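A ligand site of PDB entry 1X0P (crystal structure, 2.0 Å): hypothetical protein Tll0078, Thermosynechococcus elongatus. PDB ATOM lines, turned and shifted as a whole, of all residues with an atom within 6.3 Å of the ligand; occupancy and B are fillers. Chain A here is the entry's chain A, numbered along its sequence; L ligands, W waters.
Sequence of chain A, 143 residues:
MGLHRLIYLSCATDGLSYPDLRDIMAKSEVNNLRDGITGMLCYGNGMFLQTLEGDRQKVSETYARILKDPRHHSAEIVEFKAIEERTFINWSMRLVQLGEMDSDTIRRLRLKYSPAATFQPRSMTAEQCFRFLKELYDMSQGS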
ATOM      1  N   TYR A   8       5.799  -9.019 -28.508  1.00  0.00           N
ATOM      2  CA  TYR A   8       5.555  -9.902 -27.367  1.00  0.00           C
ATOM      3  C   TYR A   8       4.808 -11.136 -27.861  1.00  0.00           C
ATOM      4  O   TYR A   8       4.282 -11.144 -28.966  1.00  0.00           O
ATOM      5  CB  TYR A   8       4.743  -9.149 -26.286  1.00  0.00           C
ATOM      6  CG  TYR A   8       3.259  -9.033 -26.565  1.00  0.00           C
ATOM      7  CD1 TYR A   8       2.400 -10.089 -26.244  1.00  0.00           C
ATOM      8  CD2 TYR A   8       2.729  -7.924 -27.218  1.00  0.00           C
ATOM      9  CE1 TYR A   8       1.055 -10.046 -26.599  1.00  0.00           C
ATOM     10  CE2 TYR A   8       1.385  -7.872 -27.575  1.00  0.00           C
ATOM     11  CZ  TYR A   8       0.551  -8.943 -27.266  1.00  0.00           C
ATOM     12  OH  TYR A   8      -0.759  -8.952 -27.663  1.00  0.00           O
ATOM     13  N   SER A  10       2.270 -14.686 -26.378  1.00  0.00           N
ATOM     14  CA  SER A  10       1.390 -15.127 -25.304  1.00  0.00           C
ATOM     15  C   SER A  10       0.707 -16.423 -25.719  1.00  0.00           C
ATOM     16  O   SER A  10       0.786 -16.822 -26.878  1.00  0.00           O
ATOM     17  CB  SER A  10       0.327 -14.068 -24.988  1.00  0.00           C
ATOM     18  OG  SER A  10      -0.622 -13.961 -26.040  1.00  0.00           O
ATOM     19  N   ASP A  23     -13.403  -9.896 -32.277  1.00  0.00           N
ATOM     20  CA  ASP A  23     -13.578  -8.876 -31.254  1.00  0.00           C
ATOM     21  C   ASP A  23     -12.221  -8.243 -30.948  1.00  0.00           C
ATOM     22  O   ASP A  23     -12.068  -7.016 -30.888  1.00  0.00           O
ATOM     23  CB  ASP A  23     -14.189  -9.511 -29.994  1.00  0.00           C
ATOM     24  CG  ASP A  23     -14.470  -8.494 -28.888  1.00  0.00           C
ATOM     25  OD1 ASP A  23     -13.657  -8.439 -27.936  1.00  0.00           O
ATOM     26  OD2 ASP A  23     -15.480  -7.758 -28.971  1.00  0.00           O
ATOM     27  N   ILE A  24     -11.221  -9.094 -30.730  1.00  0.00           N
ATOM     28  CA  ILE A  24      -9.891  -8.584 -30.463  1.00  0.00           C
ATOM     29  C   ILE A  24      -9.516  -7.628 -31.588  1.00  0.00           C
ATOM     30  O   ILE A  24      -9.130  -6.488 -31.346  1.00  0.00           O
ATOM     31  CB  ILE A  24      -8.854  -9.723 -30.395  1.00  0.00           C
ATOM     32  CG1 ILE A  24      -9.056 -10.502 -29.097  1.00  0.00           C
ATOM     33  CG2 ILE A  24      -7.438  -9.165 -30.454  1.00  0.00           C
ATOM     34  CD1 ILE A  24      -8.443 -11.856 -29.093  1.00  0.00           C
ATOM     35  N   LYS A  27     -11.617  -4.128 -31.711  1.00  0.00           N
ATOM     36  CA  LYS A  27     -11.176  -3.124 -30.750  1.00  0.00           C
ATOM     37  C   LYS A  27      -9.761  -2.609 -31.002  1.00  0.00           C
ATOM     38  O   LYS A  27      -9.500  -1.410 -30.863  1.00  0.00           O
ATOM     39  CB  LYS A  27     -11.290  -3.655 -29.313  1.00  0.00           C
ATOM     40  CG  LYS A  27     -12.754  -3.757 -28.838  1.00  0.00           C
ATOM     41  CD  LYS A  27     -12.863  -4.025 -27.333  1.00  0.00           C
ATOM     42  CE  LYS A  27     -12.399  -5.434 -26.967  1.00  0.00           C
ATOM     43  NZ  LYS A  27     -12.611  -5.785 -25.527  1.00  0.00           N
ATOM     44  N   SER A  28      -8.861  -3.516 -31.380  1.00  0.00           N
ATOM     45  CA  SER A  28      -7.460  -3.164 -31.654  1.00  0.00           C
ATOM     46  C   SER A  28      -7.373  -2.117 -32.746  1.00  0.00           C
ATOM     47  O   SER A  28      -6.642  -1.139 -32.614  1.00  0.00           O
ATOM     48  CB  SER A  28      -6.687  -4.406 -32.100  1.00  0.00           C
ATOM     49  OG  SER A  28      -6.707  -5.405 -31.117  1.00  0.00           O
ATOM     50  N   GLU A  29      -8.106  -2.343 -33.818  1.00  0.00           N
ATOM     51  CA  GLU A  29      -8.099  -1.441 -34.952  1.00  0.00           C
ATOM     52  C   GLU A  29      -8.581  -0.049 -34.549  1.00  0.00           C
ATOM     53  O   GLU A  29      -7.963   0.961 -34.905  1.00  0.00           O
ATOM     54  CB  GLU A  29      -8.967  -2.029 -36.076  1.00  0.00           C
ATOM     55  CG  GLU A  29      -8.213  -3.043 -36.943  1.00  0.00           C
ATOM     56  CD  GLU A  29      -9.073  -4.188 -37.445  1.00  0.00           C
ATOM     57  OE1 GLU A  29     -10.252  -3.967 -37.785  1.00  0.00           O
ATOM     58  OE2 GLU A  29      -8.573  -5.330 -37.522  1.00  0.00           O
ATOM     59  N   VAL A  30      -9.658   0.006 -33.781  1.00  0.00           N
ATOM     60  CA  VAL A  30     -10.194   1.281 -33.320  1.00  0.00           C
ATOM     61  C   VAL A  30      -9.219   1.974 -32.364  1.00  0.00           C
ATOM     62  O   VAL A  30      -8.901   3.157 -32.533  1.00  0.00           O
ATOM     63  CB  VAL A  30     -11.541   1.081 -32.576  1.00  0.00           C
ATOM     64  CG1 VAL A  30     -12.024   2.403 -31.998  1.00  0.00           C
ATOM     65  CG2 VAL A  30     -12.583   0.530 -33.544  1.00  0.00           C
ATOM     66  N   ASN A  31      -8.743   1.253 -31.359  1.00  0.00           N
ATOM     67  CA  ASN A  31      -7.835   1.845 -30.396  1.00  0.00           C
ATOM     68  C   ASN A  31      -6.503   2.247 -31.023  1.00  0.00           C
ATOM     69  O   ASN A  31      -6.011   3.353 -30.829  1.00  0.00           O
ATOM     70  CB  ASN A  31      -7.578   0.885 -29.226  1.00  0.00           C
ATOM     71  CG  ASN A  31      -8.819   0.678 -28.392  1.00  0.00           C
ATOM     72  OD1 ASN A  31      -9.661   1.561 -28.298  1.00  0.00           O
ATOM     73  ND2 ASN A  31      -8.914  -0.474 -27.752  1.00  0.00           N
ATOM     74  N   ASN A  32      -5.923   1.343 -31.807  1.00  0.00           N
ATOM     75  CA  ASN A  32      -4.653   1.643 -32.419  1.00  0.00           C
ATOM     76  C   ASN A  32      -4.731   2.859 -33.353  1.00  0.00           C
ATOM     77  O   ASN A  32      -3.858   3.731 -33.321  1.00  0.00           O
ATOM     78  CB  ASN A  32      -4.132   0.398 -33.148  1.00  0.00           C
ATOM     79  CG  ASN A  32      -3.684  -0.678 -32.174  1.00  0.00           C
ATOM     80  OD1 ASN A  32      -3.751  -0.498 -30.946  1.00  0.00           O
ATOM     81  ND2 ASN A  32      -3.205  -1.789 -32.699  1.00  0.00           N
ATOM     82  N   ARG A  34      -6.685   5.286 -33.125  1.00  0.00           N
ATOM     83  CA  ARG A  34      -6.788   6.404 -32.204  1.00  0.00           C
ATOM     84  C   ARG A  34      -5.414   6.752 -31.623  1.00  0.00           C
ATOM     85  O   ARG A  34      -4.995   7.906 -31.642  1.00  0.00           O
ATOM     86  CB  ARG A  34      -7.727   6.034 -31.053  1.00  0.00           C
ATOM     87  CG  ARG A  34      -7.896   7.100 -29.978  1.00  0.00           C
ATOM     88  CD  ARG A  34      -8.502   6.495 -28.721  1.00  0.00           C
ATOM     89  NE  ARG A  34      -7.580   5.521 -28.110  1.00  0.00           N
ATOM     90  CZ  ARG A  34      -7.945   4.595 -27.232  1.00  0.00           C
ATOM     91  NH1 ARG A  34      -9.212   4.501 -26.847  1.00  0.00           N
ATOM     92  NH2 ARG A  34      -7.042   3.752 -26.752  1.00  0.00           N
ATOM     93  N   ASP A  35      -4.724   5.741 -31.122  1.00  0.00           N
ATOM     94  CA  ASP A  35      -3.434   5.955 -30.490  1.00  0.00           C
ATOM     95  C   ASP A  35      -2.236   6.148 -31.415  1.00  0.00           C
ATOM     96  O   ASP A  35      -1.110   6.339 -30.942  1.00  0.00           O
ATOM     97  CB  ASP A  35      -3.155   4.816 -29.499  1.00  0.00           C
ATOM     98  CG  ASP A  35      -4.169   4.760 -28.384  1.00  0.00           C
ATOM     99  OD1 ASP A  35      -4.735   5.830 -28.061  1.00  0.00           O
ATOM    100  OD2 ASP A  35      -4.395   3.659 -27.833  1.00  0.00           O
ATOM    101  N   ILE A  37      -1.069   3.864 -33.362  1.00  0.00           N
ATOM    102  CA  ILE A  37      -0.338   2.608 -33.313  1.00  0.00           C
ATOM    103  C   ILE A  37      -0.651   1.725 -34.534  1.00  0.00           C
ATOM    104  O   ILE A  37      -1.781   1.707 -35.022  1.00  0.00           O
ATOM    105  CB  ILE A  37      -0.687   1.844 -32.012  1.00  0.00           C
ATOM    106  CG1 ILE A  37      -0.052   2.570 -30.819  1.00  0.00           C
ATOM    107  CG2 ILE A  37      -0.236   0.406 -32.075  1.00  0.00           C
ATOM    108  CD1 ILE A  37      -0.457   2.004 -29.470  1.00  0.00           C
ATOM    109  N   LEU A  41      -0.550  -9.077 -35.960  1.00  0.00           N
ATOM    110  CA  LEU A  41      -0.896 -10.075 -34.976  1.00  0.00           C
ATOM    111  C   LEU A  41      -0.822 -11.426 -35.667  1.00  0.00           C
ATOM    112  O   LEU A  41      -1.368 -11.612 -36.755  1.00  0.00           O
ATOM    113  CB  LEU A  41      -2.298  -9.829 -34.409  1.00  0.00           C
ATOM    114  CG  LEU A  41      -2.800 -10.844 -33.360  1.00  0.00           C
ATOM    115  CD1 LEU A  41      -1.845 -10.896 -32.174  1.00  0.00           C
ATOM    116  CD2 LEU A  41      -4.189 -10.439 -32.897  1.00  0.00           C
ATOM    117  N   PHE A  48       0.091 -16.572 -29.606  1.00  0.00           N
ATOM    118  CA  PHE A  48       0.001 -15.262 -30.203  1.00  0.00           C
ATOM    119  C   PHE A  48       1.403 -14.644 -30.291  1.00  0.00           C
ATOM    120  O   PHE A  48       2.221 -14.797 -29.370  1.00  0.00           O
ATOM    121  CB  PHE A  48      -0.862 -14.354 -29.340  1.00  0.00           C
ATOM    122  CG  PHE A  48      -2.330 -14.546 -29.527  1.00  0.00           C
ATOM    123  CD1 PHE A  48      -3.146 -14.925 -28.446  1.00  0.00           C
ATOM    124  CD2 PHE A  48      -2.914 -14.326 -30.767  1.00  0.00           C
ATOM    125  CE1 PHE A  48      -4.531 -15.078 -28.624  1.00  0.00           C
ATOM    126  CE2 PHE A  48      -4.288 -14.472 -30.950  1.00  0.00           C
ATOM    127  CZ  PHE A  48      -5.098 -14.843 -29.884  1.00  0.00           C
ATOM    128  N   GLN A  50       2.705 -10.846 -31.473  1.00  0.00           N
ATOM    129  CA  GLN A  50       2.258  -9.556 -31.948  1.00  0.00           C
ATOM    130  C   GLN A  50       3.310  -8.470 -31.851  1.00  0.00           C
ATOM    131  O   GLN A  50       4.211  -8.515 -31.015  1.00  0.00           O
ATOM    132  CB  GLN A  50       1.023  -9.102 -31.125  1.00  0.00           C
ATOM    133  CG  GLN A  50       0.484  -7.712 -31.494  1.00  0.00           C
ATOM    134  CD  GLN A  50      -0.863  -7.371 -30.823  1.00  0.00           C
ATOM    135  OE1 GLN A  50      -0.985  -7.385 -29.593  1.00  0.00           O
ATOM    136  NE2 GLN A  50      -1.867  -7.030 -31.633  1.00  0.00           N
ATOM    137  N   LEU A  52       3.746  -4.092 -32.021  1.00  0.00           N
ATOM    138  CA  LEU A  52       3.105  -2.795 -32.030  1.00  0.00           C
ATOM    139  C   LEU A  52       4.148  -1.700 -32.205  1.00  0.00           C
ATOM    140  O   LEU A  52       5.201  -1.713 -31.570  1.00  0.00           O
ATOM    141  CB  LEU A  52       2.359  -2.544 -30.708  1.00  0.00           C
ATOM    142  CG  LEU A  52       1.254  -3.504 -30.262  1.00  0.00           C
ATOM    143  CD1 LEU A  52       0.693  -3.053 -28.901  1.00  0.00           C
ATOM    144  CD2 LEU A  52       0.144  -3.521 -31.300  1.00  0.00           C
ATOM    145  N   THR A  62      -1.039   0.366 -24.082  1.00  0.00           N
ATOM    146  CA  THR A  62      -1.781  -0.645 -24.827  1.00  0.00           C
ATOM    147  C   THR A  62      -1.355  -2.033 -24.349  1.00  0.00           C
ATOM    148  O   THR A  62      -2.194  -2.930 -24.204  1.00  0.00           O
ATOM    149  CB  THR A  62      -1.556  -0.511 -26.361  1.00  0.00           C
ATOM    150  OG1 THR A  62      -2.164   0.705 -26.823  1.00  0.00           O
ATOM    151  CG2 THR A  62      -2.170  -1.675 -27.105  1.00  0.00           C
ATOM    152  N   ARG A  65      -2.862  -2.887 -21.047  1.00  0.00           N
ATOM    153  CA  ARG A  65      -4.275  -3.202 -21.250  1.00  0.00           C
ATOM    154  C   ARG A  65      -4.408  -4.639 -21.752  1.00  0.00           C
ATOM    155  O   ARG A  65      -5.254  -5.406 -21.297  1.00  0.00           O
ATOM    156  CB  ARG A  65      -4.850  -2.222 -22.264  1.00  0.00           C
ATOM    157  CG  ARG A  65      -6.228  -1.693 -21.937  1.00  0.00           C
ATOM    158  CD  ARG A  65      -6.484  -0.395 -22.681  1.00  0.00           C
ATOM    159  NE  ARG A  65      -6.321  -0.546 -24.125  1.00  0.00           N
ATOM    160  CZ  ARG A  65      -5.582   0.251 -24.889  1.00  0.00           C
ATOM    161  NH1 ARG A  65      -4.924   1.263 -24.337  1.00  0.00           N
ATOM    162  NH2 ARG A  65      -5.503   0.049 -26.191  1.00  0.00           N
ATOM    163  N   ILE A  66      -3.539  -5.006 -22.681  1.00  0.00           N
ATOM    164  CA  ILE A  66      -3.522  -6.343 -23.248  1.00  0.00           C
ATOM    165  C   ILE A  66      -3.264  -7.386 -22.168  1.00  0.00           C
ATOM    166  O   ILE A  66      -3.851  -8.476 -22.183  1.00  0.00           O
ATOM    167  CB  ILE A  66      -2.417  -6.452 -24.341  1.00  0.00           C
ATOM    168  CG1 ILE A  66      -2.804  -5.586 -25.539  1.00  0.00           C
ATOM    169  CG2 ILE A  66      -2.193  -7.895 -24.747  1.00  0.00           C
ATOM    170  CD1 ILE A  66      -1.713  -5.440 -26.573  1.00  0.00           C
ATOM    171  N   LEU A  67      -2.393  -7.066 -21.222  1.00  0.00           N
ATOM    172  CA  LEU A  67      -2.082  -8.007 -20.152  1.00  0.00           C
ATOM    173  C   LEU A  67      -3.282  -8.350 -19.291  1.00  0.00           C
ATOM    174  O   LEU A  67      -3.308  -9.413 -18.670  1.00  0.00           O
ATOM    175  CB  LEU A  67      -0.970  -7.455 -19.246  1.00  0.00           C
ATOM    176  CG  LEU A  67       0.452  -7.418 -19.810  1.00  0.00           C
ATOM    177  CD1 LEU A  67       1.377  -6.798 -18.765  1.00  0.00           C
ATOM    178  CD2 LEU A  67       0.912  -8.822 -20.165  1.00  0.00           C
ATOM    179  N   LYS A  68      -4.277  -7.470 -19.260  1.00  0.00           N
ATOM    180  CA  LYS A  68      -5.481  -7.697 -18.457  1.00  0.00           C
ATOM    181  C   LYS A  68      -6.525  -8.498 -19.222  1.00  0.00           C
ATOM    182  O   LYS A  68      -7.572  -8.833 -18.678  1.00  0.00           O
ATOM    183  CB  LYS A  68      -6.075  -6.354 -18.024  1.00  0.00           C
ATOM    184  CG  LYS A  68      -5.170  -5.517 -17.147  1.00  0.00           C
ATOM    185  CD  LYS A  68      -5.723  -4.125 -16.933  1.00  0.00           C
ATOM    186  CE  LYS A  68      -4.759  -3.268 -16.148  1.00  0.00           C
ATOM    187  NZ  LYS A  68      -5.304  -1.886 -15.915  1.00  0.00           N
ATOM    188  N   ASP A  69      -6.248  -8.798 -20.485  1.00  0.00           N
ATOM    189  CA  ASP A  69      -7.184  -9.562 -21.301  1.00  0.00           C
ATOM    190  C   ASP A  69      -7.168 -11.047 -20.909  1.00  0.00           C
ATOM    191  O   ASP A  69      -6.144 -11.714 -20.997  1.00  0.00           O
ATOM    192  CB  ASP A  69      -6.834  -9.431 -22.778  1.00  0.00           C
ATOM    193  CG  ASP A  69      -7.996  -9.740 -23.686  1.00  0.00           C
ATOM    194  OD1 ASP A  69      -8.657 -10.781 -23.477  1.00  0.00           O
ATOM    195  OD2 ASP A  69      -8.249  -8.945 -24.612  1.00  0.00           O
ATOM    196  N   ARG A  71      -8.463 -13.523 -22.436  1.00  0.00           N
ATOM    197  CA  ARG A  71      -8.407 -14.408 -23.602  1.00  0.00           C
ATOM    198  C   ARG A  71      -7.011 -14.963 -23.950  1.00  0.00           C
ATOM    199  O   ARG A  71      -6.838 -15.712 -24.921  1.00  0.00           O
ATOM    200  CB  ARG A  71      -9.027 -13.710 -24.812  1.00  0.00           C
ATOM    201  CG  ARG A  71     -10.555 -13.524 -24.655  1.00  0.00           C
ATOM    202  CD  ARG A  71     -11.135 -12.508 -25.632  1.00  0.00           C
ATOM    203  NE  ARG A  71     -10.585 -11.157 -25.455  1.00  0.00           N
ATOM    204  CZ  ARG A  71     -11.045 -10.076 -26.077  1.00  0.00           C
ATOM    205  NH1 ARG A  71     -12.064 -10.167 -26.923  1.00  0.00           N
ATOM    206  NH2 ARG A  71     -10.473  -8.900 -25.873  1.00  0.00           N
ATOM    207  N   HIS A  72      -6.015 -14.590 -23.156  1.00  0.00           N
ATOM    208  CA  HIS A  72      -4.663 -15.118 -23.342  1.00  0.00           C
ATOM    209  C   HIS A  72      -3.945 -15.012 -22.016  1.00  0.00           C
ATOM    210  O   HIS A  72      -4.418 -14.336 -21.114  1.00  0.00           O
ATOM    211  CB  HIS A  72      -3.885 -14.411 -24.458  1.00  0.00           C
ATOM    212  CG  HIS A  72      -3.530 -12.984 -24.161  1.00  0.00           C
ATOM    213  ND1 HIS A  72      -2.514 -12.320 -24.813  1.00  0.00           N
ATOM    214  CD2 HIS A  72      -4.074 -12.097 -23.305  1.00  0.00           C
ATOM    215  CE1 HIS A  72      -2.455 -11.071 -24.366  1.00  0.00           C
ATOM    216  NE2 HIS A  72      -3.391 -10.910 -23.451  1.00  0.00           N
ATOM    217  N   SER A  92      -3.675  -0.598 -38.800  1.00  0.00           N
ATOM    218  CA  SER A  92      -3.768  -0.237 -37.380  1.00  0.00           C
ATOM    219  C   SER A  92      -3.494  -1.585 -36.690  1.00  0.00           C
ATOM    220  O   SER A  92      -2.888  -1.655 -35.617  1.00  0.00           O
ATOM    221  CB  SER A  92      -5.169   0.286 -37.051  1.00  0.00           C
ATOM    222  OG  SER A  92      -6.144  -0.645 -37.449  1.00  0.00           O
ATOM    223  N   MET A  93      -3.965  -2.647 -37.323  1.00  0.00           N
ATOM    224  CA  MET A  93      -3.699  -4.005 -36.893  1.00  0.00           C
ATOM    225  C   MET A  93      -4.186  -4.927 -37.992  1.00  0.00           C
ATOM    226  O   MET A  93      -5.162  -4.629 -38.690  1.00  0.00           O
ATOM    227  CB  MET A  93      -4.362  -4.347 -35.554  1.00  0.00           C
ATOM    228  CG  MET A  93      -3.905  -5.717 -34.967  1.00  0.00           C
ATOM    229  SD  MET A  93      -2.074  -6.025 -34.970  1.00  0.00           S
ATOM    230  CE  MET A  93      -1.450  -4.632 -34.009  1.00  0.00           C
HETATM  231  N1  LIG L   1      -6.144  -3.894 -27.929  1.00  0.00           N
HETATM  232  C1  LIG L   1      -5.715  -2.725 -28.563  1.00  0.00           C
HETATM  233  O1  LIG L   1      -6.212  -1.634 -28.314  1.00  0.00           O
HETATM  234  N2  LIG L   1      -4.658  -2.919 -29.499  1.00  0.00           N
HETATM  235  C2  LIG L   1      -4.029  -4.153 -29.830  1.00  0.00           C
HETATM  236  O2  LIG L   1      -3.155  -4.184 -30.679  1.00  0.00           O
HETATM  237  C3  LIG L   1      -4.562  -5.284 -29.104  1.00  0.00           C
HETATM  238  N3  LIG L   1      -3.955  -6.522 -29.410  1.00  0.00           N
HETATM  239  C4  LIG L   1      -4.418  -7.660 -28.724  1.00  0.00           C
HETATM  240  C5  LIG L   1      -3.812  -8.876 -29.019  1.00  0.00           C
HETATM  241  C6  LIG L   1      -4.239 -10.033 -28.364  1.00  0.00           C
HETATM  242  C7  LIG L   1      -3.575 -11.362 -28.677  1.00  0.00           C
HETATM  243  C8  LIG L   1      -5.323  -9.962 -27.385  1.00  0.00           C
HETATM  244  C9  LIG L   1      -5.806 -11.224 -26.661  1.00  0.00           C
HETATM  245  C10 LIG L   1      -5.933  -8.736 -27.100  1.00  0.00           C
HETATM  246  C11 LIG L   1      -5.500  -7.569 -27.747  1.00  0.00           C
HETATM  247  N4  LIG L   1      -6.105  -6.314 -27.466  1.00  0.00           N
HETATM  248  C12 LIG L   1      -5.642  -5.184 -28.129  1.00  0.00           C
HETATM  249  C13 LIG L   1      -7.167  -6.159 -26.525  1.00  0.00           C
HETATM  250  C14 LIG L   1      -7.074  -5.608 -25.226  1.00  0.00           C
HETATM  251  O3  LIG L   1      -6.623  -6.697 -24.346  1.00  0.00           O
HETATM  252  C15 LIG L   1      -8.313  -4.846 -24.893  1.00  0.00           C
HETATM  253  O4  LIG L   1      -9.418  -5.716 -24.714  1.00  0.00           O
HETATM  254  C16 LIG L   1      -8.673  -3.405 -25.526  1.00  0.00           C
HETATM  255  O5  LIG L   1      -7.414  -2.627 -25.663  1.00  0.00           O
HETATM  256  C17 LIG L   1      -9.580  -2.497 -24.638  1.00  0.00           C
HETATM  257  O6  LIG L   1     -10.067  -1.114 -24.909  1.00  0.00           O
HETATM  258  O   HOH W   1      -3.942   0.959 -28.709  1.00  0.00           O
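OD2 of Asp 69 sits at hydrogen-bond distance from O3 of the ligand (2.8 Å). NH2 of Arg 65 sits at hydrogen-bond distance from O1 of the ligand, at 2.8 Å. OG of Ser 28 sits close to N3 of the ligand. N2 of the ligand sits at hydrogen-bond distance from OD1 of Asn 32 (3.0 Å). The side-chain amide nitrogen (ND2) of Asn 31 lies within hydrogen-bond range of an oxygen (O1) of the ligand, 3.0 Å away. The side-chain amide nitrogen (NE2) of Gln 50 lies within hydrogen-bond range of a nitrogen (N3) of the ligand (3.1 Å). An oxygen (O4) of the ligand sits at hydrogen-bond distance from the side-chain amino group (NZ) of Lys 27 (3.3 Å).
OD2 of Asp 69 lies within salt-bridge range of NH2 of Arg 71. O of Ser 28 lies close to OD1 of Asn 32, 3.4 Å away. The side-chain hydroxyl (OG) of Ser 28 is in hydrogen-bond range of the backbone carbonyl oxygen (O) of Ile 24 (2.7 Å). The backbone carbonyl oxygen of Asn 32 is in hydrogen-bond range of the backbone NH of Ile 37 (2.8 Å). The guanidinium group (NH1) of Arg 34 sits at hydrogen-bond distance from the side-chain amide oxygen (OD1) of Asn 31 (3.3 Å). The side-chain amide nitrogen (NE2) of Gln 50 sits close to the side-chain sulfur (SD) of Met 93. The backbone carbonyl oxygen (O) of Ile 66 sits at hydrogen-bond distance from a ring nitrogen (NE2) of His 72 (2.8 Å). N of Leu 41 lies within hydrogen-bond range of SD of Met 93, 3.6 Å away.
Merely in contact with the ligand: Ile 66, Tyr 8, Leu 52, Phe 48, Arg 71, Ile 24, Thr 62, Met 93, His 72 and Leu 41. Hydrophobic or aromatic side chains that line the ligand: Ile 24, Leu 41, Phe 48, Leu 52, Ile 66, His 72 and Met 93. 17 residues have an atom within 4 Å of the ligand: Tyr 8, Ile 24, Lys 27, Ser 28, Asn 31, Asn 32, Leu 41, Phe 48, Gln 50, Leu 52, Thr 62, Arg 65, Ile 66, Asp 69, Arg 71, His 72 and Met 93.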
